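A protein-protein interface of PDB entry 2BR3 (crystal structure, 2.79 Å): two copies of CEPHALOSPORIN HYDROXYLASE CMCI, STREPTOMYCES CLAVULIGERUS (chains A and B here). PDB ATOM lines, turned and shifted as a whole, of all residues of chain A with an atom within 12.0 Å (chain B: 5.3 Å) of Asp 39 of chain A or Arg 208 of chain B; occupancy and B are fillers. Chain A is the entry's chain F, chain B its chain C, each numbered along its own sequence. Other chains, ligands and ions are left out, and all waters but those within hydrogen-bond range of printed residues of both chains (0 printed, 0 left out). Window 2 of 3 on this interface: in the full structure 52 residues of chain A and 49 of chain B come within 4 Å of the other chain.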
ATOM      1  N   PRO A  33      11.895  12.137   7.713  1.00  0.00           N
ATOM      2  CA  PRO A  33      11.096  10.913   7.625  1.00  0.00           C
ATOM      3  C   PRO A  33      11.101  10.399   6.196  1.00  0.00           C
ATOM      4  O   PRO A  33      11.328  11.178   5.276  1.00  0.00           O
ATOM      5  CB  PRO A  33       9.691  11.381   8.010  1.00  0.00           C
ATOM      6  CG  PRO A  33       9.655  12.826   7.638  1.00  0.00           C
ATOM      7  CD  PRO A  33      11.051  13.335   7.892  1.00  0.00           C
ATOM      8  N   ARG A  34      10.864   9.109   6.014  1.00  0.00           N
ATOM      9  CA  ARG A  34      10.747   8.551   4.678  1.00  0.00           C
ATOM     10  C   ARG A  34       9.393   8.907   4.092  1.00  0.00           C
ATOM     11  O   ARG A  34       9.276   9.120   2.888  1.00  0.00           O
ATOM     12  CB  ARG A  34      10.923   7.033   4.681  1.00  0.00           C
ATOM     13  CG  ARG A  34      11.108   6.460   3.285  1.00  0.00           C
ATOM     14  CD  ARG A  34      11.240   4.951   3.236  1.00  0.00           C
ATOM     15  NE  ARG A  34      10.869   4.436   1.919  1.00  0.00           N
ATOM     16  CZ  ARG A  34      11.332   3.313   1.387  1.00  0.00           C
ATOM     17  NH1 ARG A  34      12.177   2.538   2.054  1.00  0.00           N
ATOM     18  NH2 ARG A  34      10.938   2.947   0.178  1.00  0.00           N
ATOM     19  N   ASP A  35       8.376   8.964   4.947  1.00  0.00           N
ATOM     20  CA  ASP A  35       7.024   9.284   4.509  1.00  0.00           C
ATOM     21  C   ASP A  35       6.744  10.737   4.831  1.00  0.00           C
ATOM     22  O   ASP A  35       6.690  11.118   5.995  1.00  0.00           O
ATOM     23  CB  ASP A  35       6.010   8.377   5.200  1.00  0.00           C
ATOM     24  CG  ASP A  35       6.364   6.912   5.069  1.00  0.00           C
ATOM     25  OD1 ASP A  35       5.610   6.171   4.399  1.00  0.00           O
ATOM     26  OD2 ASP A  35       7.391   6.420   5.593  1.00  0.00           O
ATOM     27  N   TRP A  36       6.581  11.547   3.789  1.00  0.00           N
ATOM     28  CA  TRP A  36       6.398  12.977   3.954  1.00  0.00           C
ATOM     29  C   TRP A  36       4.905  13.335   3.882  1.00  0.00           C
ATOM     30  O   TRP A  36       4.189  12.856   2.993  1.00  0.00           O
ATOM     31  CB  TRP A  36       7.205  13.757   2.908  1.00  0.00           C
ATOM     32  CG  TRP A  36       7.240  15.213   3.215  1.00  0.00           C
ATOM     33  CD1 TRP A  36       6.350  16.149   2.794  1.00  0.00           C
ATOM     34  CD2 TRP A  36       8.177  15.900   4.052  1.00  0.00           C
ATOM     35  NE1 TRP A  36       6.681  17.382   3.301  1.00  0.00           N
ATOM     36  CE2 TRP A  36       7.800  17.260   4.077  1.00  0.00           C
ATOM     37  CE3 TRP A  36       9.309  15.509   4.775  1.00  0.00           C
ATOM     38  CZ2 TRP A  36       8.509  18.231   4.795  1.00  0.00           C
ATOM     39  CZ3 TRP A  36      10.019  16.477   5.489  1.00  0.00           C
ATOM     40  CH2 TRP A  36       9.611  17.821   5.491  1.00  0.00           C
ATOM     41  N   PRO A  37       4.434  14.170   4.811  1.00  0.00           N
ATOM     42  CA  PRO A  37       3.015  14.538   4.844  1.00  0.00           C
ATOM     43  C   PRO A  37       2.640  15.333   3.607  1.00  0.00           C
ATOM     44  O   PRO A  37       3.300  16.320   3.313  1.00  0.00           O
ATOM     45  CB  PRO A  37       2.891  15.414   6.102  1.00  0.00           C
ATOM     46  CG  PRO A  37       4.172  15.272   6.843  1.00  0.00           C
ATOM     47  CD  PRO A  37       5.203  14.841   5.876  1.00  0.00           C
ATOM     48  N   LEU A  38       1.597  14.908   2.902  1.00  0.00           N
ATOM     49  CA  LEU A  38       1.203  15.541   1.644  1.00  0.00           C
ATOM     50  C   LEU A  38       0.510  16.895   1.851  1.00  0.00           C
ATOM     51  O   LEU A  38       0.383  17.681   0.919  1.00  0.00           O
ATOM     52  CB  LEU A  38       0.314  14.588   0.826  1.00  0.00           C
ATOM     53  CG  LEU A  38       0.929  13.989  -0.448  1.00  0.00           C
ATOM     54  CD1 LEU A  38       2.289  13.380  -0.193  1.00  0.00           C
ATOM     55  CD2 LEU A  38      -0.009  12.946  -1.062  1.00  0.00           C
ATOM     56  N   ASP A  39       0.061  17.183   3.062  1.00  0.00           N
ATOM     57  CA  ASP A  39      -0.475  18.513   3.340  1.00  0.00           C
ATOM     58  C   ASP A  39       0.637  19.554   3.501  1.00  0.00           C
ATOM     59  O   ASP A  39       0.380  20.751   3.394  1.00  0.00           O
ATOM     60  CB  ASP A  39      -1.442  18.501   4.538  1.00  0.00           C
ATOM     61  CG  ASP A  39      -0.759  18.235   5.857  1.00  0.00           C
ATOM     62  OD1 ASP A  39       0.037  17.285   5.951  1.00  0.00           O
ATOM     63  OD2 ASP A  39      -0.979  18.925   6.868  1.00  0.00           O
ATOM     64  N   ARG A  40       1.860  19.091   3.757  1.00  0.00           N
ATOM     65  CA  ARG A  40       3.038  19.954   3.809  1.00  0.00           C
ATOM     66  C   ARG A  40       3.975  19.655   2.634  1.00  0.00           C
ATOM     67  O   ARG A  40       5.176  19.915   2.707  1.00  0.00           O
ATOM     68  CB  ARG A  40       3.772  19.780   5.151  1.00  0.00           C
ATOM     69  CG  ARG A  40       3.111  20.524   6.319  1.00  0.00           C
ATOM     70  CD  ARG A  40       3.761  20.308   7.708  1.00  0.00           C
ATOM     71  NE  ARG A  40       2.895  20.818   8.787  1.00  0.00           N
ATOM     72  CZ  ARG A  40       3.128  20.699  10.101  1.00  0.00           C
ATOM     73  NH1 ARG A  40       4.218  20.081  10.552  1.00  0.00           N
ATOM     74  NH2 ARG A  40       2.262  21.210  10.975  1.00  0.00           N
ATOM     75  N   TRP A  41       3.423  19.143   1.534  1.00  0.00           N
ATOM     76  CA  TRP A  41       4.227  18.702   0.387  1.00  0.00           C
ATOM     77  C   TRP A  41       5.238  19.742  -0.107  1.00  0.00           C
ATOM     78  O   TRP A  41       6.382  19.403  -0.386  1.00  0.00           O
ATOM     79  CB  TRP A  41       3.312  18.287  -0.757  1.00  0.00           C
ATOM     80  CG  TRP A  41       4.018  17.954  -2.029  1.00  0.00           C
ATOM     81  CD1 TRP A  41       4.482  16.732  -2.414  1.00  0.00           C
ATOM     82  CD2 TRP A  41       4.314  18.852  -3.103  1.00  0.00           C
ATOM     83  NE1 TRP A  41       5.053  16.817  -3.660  1.00  0.00           N
ATOM     84  CE2 TRP A  41       4.963  18.111  -4.104  1.00  0.00           C
ATOM     85  CE3 TRP A  41       4.101  20.218  -3.317  1.00  0.00           C
ATOM     86  CZ2 TRP A  41       5.405  18.690  -5.297  1.00  0.00           C
ATOM     87  CZ3 TRP A  41       4.533  20.789  -4.503  1.00  0.00           C
ATOM     88  CH2 TRP A  41       5.180  20.030  -5.474  1.00  0.00           C
ATOM     89  N   ALA A  42       4.819  21.001  -0.202  1.00  0.00           N
ATOM     90  CA  ALA A  42       5.680  22.076  -0.699  1.00  0.00           C
ATOM     91  C   ALA A  42       6.926  22.345   0.154  1.00  0.00           C
ATOM     92  O   ALA A  42       7.907  22.883  -0.355  1.00  0.00           O
ATOM     93  CB  ALA A  42       4.875  23.355  -0.846  1.00  0.00           C
ATOM     94  N   GLU A  43       6.893  21.985   1.437  1.00  0.00           N
ATOM     95  CA  GLU A  43       8.039  22.210   2.339  1.00  0.00           C
ATOM     96  C   GLU A  43       9.157  21.159   2.232  1.00  0.00           C
ATOM     97  O   GLU A  43      10.223  21.333   2.826  1.00  0.00           O
ATOM     98  CB  GLU A  43       7.575  22.262   3.802  1.00  0.00           C
ATOM     99  CG  GLU A  43       6.792  23.499   4.201  1.00  0.00           C
ATOM    100  CD  GLU A  43       6.188  23.366   5.596  1.00  0.00           C
ATOM    101  OE1 GLU A  43       6.953  23.249   6.582  1.00  0.00           O
ATOM    102  OE2 GLU A  43       4.944  23.363   5.712  1.00  0.00           O
ATOM    103  N   ALA A  44       8.917  20.075   1.494  1.00  0.00           N
ATOM    104  CA  ALA A  44       9.794  18.906   1.558  1.00  0.00           C
ATOM    105  C   ALA A  44      11.128  19.171   0.875  1.00  0.00           C
ATOM    106  O   ALA A  44      11.159  19.720  -0.230  1.00  0.00           O
ATOM    107  CB  ALA A  44       9.124  17.699   0.939  1.00  0.00           C
ATOM    108  N   PRO A  45      12.222  18.758   1.515  1.00  0.00           N
ATOM    109  CA  PRO A  45      13.562  19.050   1.006  1.00  0.00           C
ATOM    110  C   PRO A  45      13.779  18.425  -0.367  1.00  0.00           C
ATOM    111  O   PRO A  45      13.290  17.313  -0.624  1.00  0.00           O
ATOM    112  CB  PRO A  45      14.484  18.412   2.056  1.00  0.00           C
ATOM    113  CG  PRO A  45      13.670  17.387   2.710  1.00  0.00           C
ATOM    114  CD  PRO A  45      12.277  17.942   2.739  1.00  0.00           C
ATOM    115  N   LEU B 204      -3.555  17.794  -3.754  1.00  0.00           N
ATOM    116  CA  LEU B 204      -2.647  16.817  -3.145  1.00  0.00           C
ATOM    117  C   LEU B 204      -2.846  16.739  -1.628  1.00  0.00           C
ATOM    118  O   LEU B 204      -2.699  15.668  -1.039  1.00  0.00           O
ATOM    119  CB  LEU B 204      -1.173  17.149  -3.450  1.00  0.00           C
ATOM    120  CG  LEU B 204      -0.323  16.214  -4.333  1.00  0.00           C
ATOM    121  CD1 LEU B 204       1.148  16.296  -3.910  1.00  0.00           C
ATOM    122  CD2 LEU B 204      -0.781  14.760  -4.323  1.00  0.00           C
ATOM    123  N   GLY B 205      -3.172  17.873  -1.010  1.00  0.00           N
ATOM    124  CA  GLY B 205      -3.354  17.954   0.426  1.00  0.00           C
ATOM    125  C   GLY B 205      -4.470  17.047   0.898  1.00  0.00           C
ATOM    126  O   GLY B 205      -4.378  16.447   1.969  1.00  0.00           O
ATOM    127  N   ALA B 206      -5.515  16.928   0.079  1.00  0.00           N
ATOM    128  CA  ALA B 206      -6.679  16.092   0.390  1.00  0.00           C
ATOM    129  C   ALA B 206      -6.327  14.618   0.654  1.00  0.00           C
ATOM    130  O   ALA B 206      -7.079  13.909   1.322  1.00  0.00           O
ATOM    131  CB  ALA B 206      -7.693  16.194  -0.740  1.00  0.00           C
ATOM    132  N   PHE B 207      -5.190  14.168   0.130  1.00  0.00           N
ATOM    133  CA  PHE B 207      -4.746  12.788   0.279  1.00  0.00           C
ATOM    134  C   PHE B 207      -3.771  12.589   1.452  1.00  0.00           C
ATOM    135  O   PHE B 207      -3.073  11.575   1.505  1.00  0.00           O
ATOM    136  CB  PHE B 207      -4.079  12.321  -1.024  1.00  0.00           C
ATOM    137  CG  PHE B 207      -5.015  12.254  -2.208  1.00  0.00           C
ATOM    138  CD1 PHE B 207      -5.326  13.396  -2.930  1.00  0.00           C
ATOM    139  CD2 PHE B 207      -5.570  11.042  -2.608  1.00  0.00           C
ATOM    140  CE1 PHE B 207      -6.189  13.337  -4.019  1.00  0.00           C
ATOM    141  CE2 PHE B 207      -6.425  10.974  -3.702  1.00  0.00           C
ATOM    142  CZ  PHE B 207      -6.734  12.119  -4.409  1.00  0.00           C
ATOM    143  N   ARG B 208      -3.729  13.528   2.399  1.00  0.00           N
ATOM    144  CA  ARG B 208      -2.799  13.433   3.527  1.00  0.00           C
ATOM    145  C   ARG B 208      -3.050  12.194   4.402  1.00  0.00           C
ATOM    146  O   ARG B 208      -2.111  11.565   4.868  1.00  0.00           O
ATOM    147  CB  ARG B 208      -2.828  14.716   4.382  1.00  0.00           C
ATOM    148  CG  ARG B 208      -4.084  14.892   5.247  1.00  0.00           C
ATOM    149  CD  ARG B 208      -4.573  16.347   5.412  1.00  0.00           C
ATOM    150  NE  ARG B 208      -5.837  16.612   4.700  1.00  0.00           N
ATOM    151  CZ  ARG B 208      -7.062  16.598   5.247  1.00  0.00           C
ATOM    152  NH1 ARG B 208      -7.245  16.343   6.543  1.00  0.00           N
ATOM    153  NH2 ARG B 208      -8.122  16.847   4.478  1.00  0.00           N
ATOM    154  N   ASP B 209      -4.312  11.831   4.600  1.00  0.00           N
ATOM    155  CA  ASP B 209      -4.656  10.714   5.490  1.00  0.00           C
ATOM    156  C   ASP B 209      -4.497   9.335   4.832  1.00  0.00           C
ATOM    157  O   ASP B 209      -4.566   8.316   5.519  1.00  0.00           O
ATOM    158  CB  ASP B 209      -6.093  10.854   6.025  1.00  0.00           C
ATOM    159  CG  ASP B 209      -6.331  12.175   6.737  1.00  0.00           C
ATOM    160  OD1 ASP B 209      -5.533  12.517   7.631  1.00  0.00           O
ATOM    161  OD2 ASP B 209      -7.281  12.940   6.467  1.00  0.00           O
ATOM    162  N   VAL B 210      -4.287   9.294   3.519  1.00  0.00           N
ATOM    163  CA  VAL B 210      -4.241   8.016   2.808  1.00  0.00           C
ATOM    164  C   VAL B 210      -3.028   7.805   1.893  1.00  0.00           C
ATOM    165  O   VAL B 210      -2.883   6.721   1.320  1.00  0.00           O
ATOM    166  CB  VAL B 210      -5.543   7.785   1.992  1.00  0.00           C
ATOM    167  CG1 VAL B 210      -6.654   7.269   2.905  1.00  0.00           C
ATOM    168  CG2 VAL B 210      -5.974   9.064   1.261  1.00  0.00           C
ATOM    169  N   LEU B 211      -2.156   8.812   1.786  1.00  0.00           N
ATOM    170  CA  LEU B 211      -0.966   8.746   0.922  1.00  0.00           C
ATOM    171  C   LEU B 211       0.183   9.603   1.447  1.00  0.00           C
ATOM    172  O   LEU B 211      -0.025  10.716   1.952  1.00  0.00           O
ATOM    173  CB  LEU B 211      -1.292   9.227  -0.492  1.00  0.00           C
ATOM    174  CG  LEU B 211      -1.985   8.293  -1.485  1.00  0.00           C
ATOM    175  CD1 LEU B 211      -2.245   9.056  -2.772  1.00  0.00           C
ATOM    176  CD2 LEU B 211      -1.173   7.034  -1.755  1.00  0.00           C
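Leu 38 of chain A touches Leu 204 of chain B. O of Leu 38 of chain A touches CA of Gly 205 of chain B, at 3.8 Å. Leu 38 of chain A touches Leu 211 of chain B (CD2 to O, 3.7 Å). Arg 208 of chain B touches Asp 39 of chain A. Trp 41 of chain A touches Leu 204 of chain B.
Of chain B, only Arg 208 (3.9 Å) comes within 4 Å of Asp 39 of chain A. Of chain A, only Asp 39 (3.9 Å) comes within 4 Å of Arg 208 of chain B. Ala 206 of chain B touches none of the printed residues of chain A. No residue of chain A comes within 4 Å of Phe 207 of chain B. No residue of chain A comes within 4 Å of Asp 209 of chain B. No residue of chain A comes within 4 Å of Val 210 of chain B. Of the printed residues of chain B, Leu 38 of chain A touches Leu 204, Gly 205 and Leu 211. Printed residues of chain B within 4 Å of Trp 41 of chain A: Leu 204. Printed residues of chain A within 4 Å of Leu 211 of chain B: Leu 38 (3.7 Å). The nearest residue of chain A that does not touch Arg 208 of chain B is Leu 38 of chain A (4.3 Å).
NH1 of Arg 208 of chain B lies within salt-bridge range of OD2 of Asp 209 of chain B. O of Gly 205 of chain B sits at hydrogen-bond distance from NE of Arg 208 of chain B (3.1 Å).
Hydrophobic or aromatic side chains of chain A that line the printed part of chain B: Leu 38 and Trp 41. Among the printed residues, 5 pairs touch across the chains. Among the printed residues, no Asp or Glu carboxylate lies within 4 Å of a Lys or Arg side-chain nitrogen of the other chain.
No position is printed for both chains.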
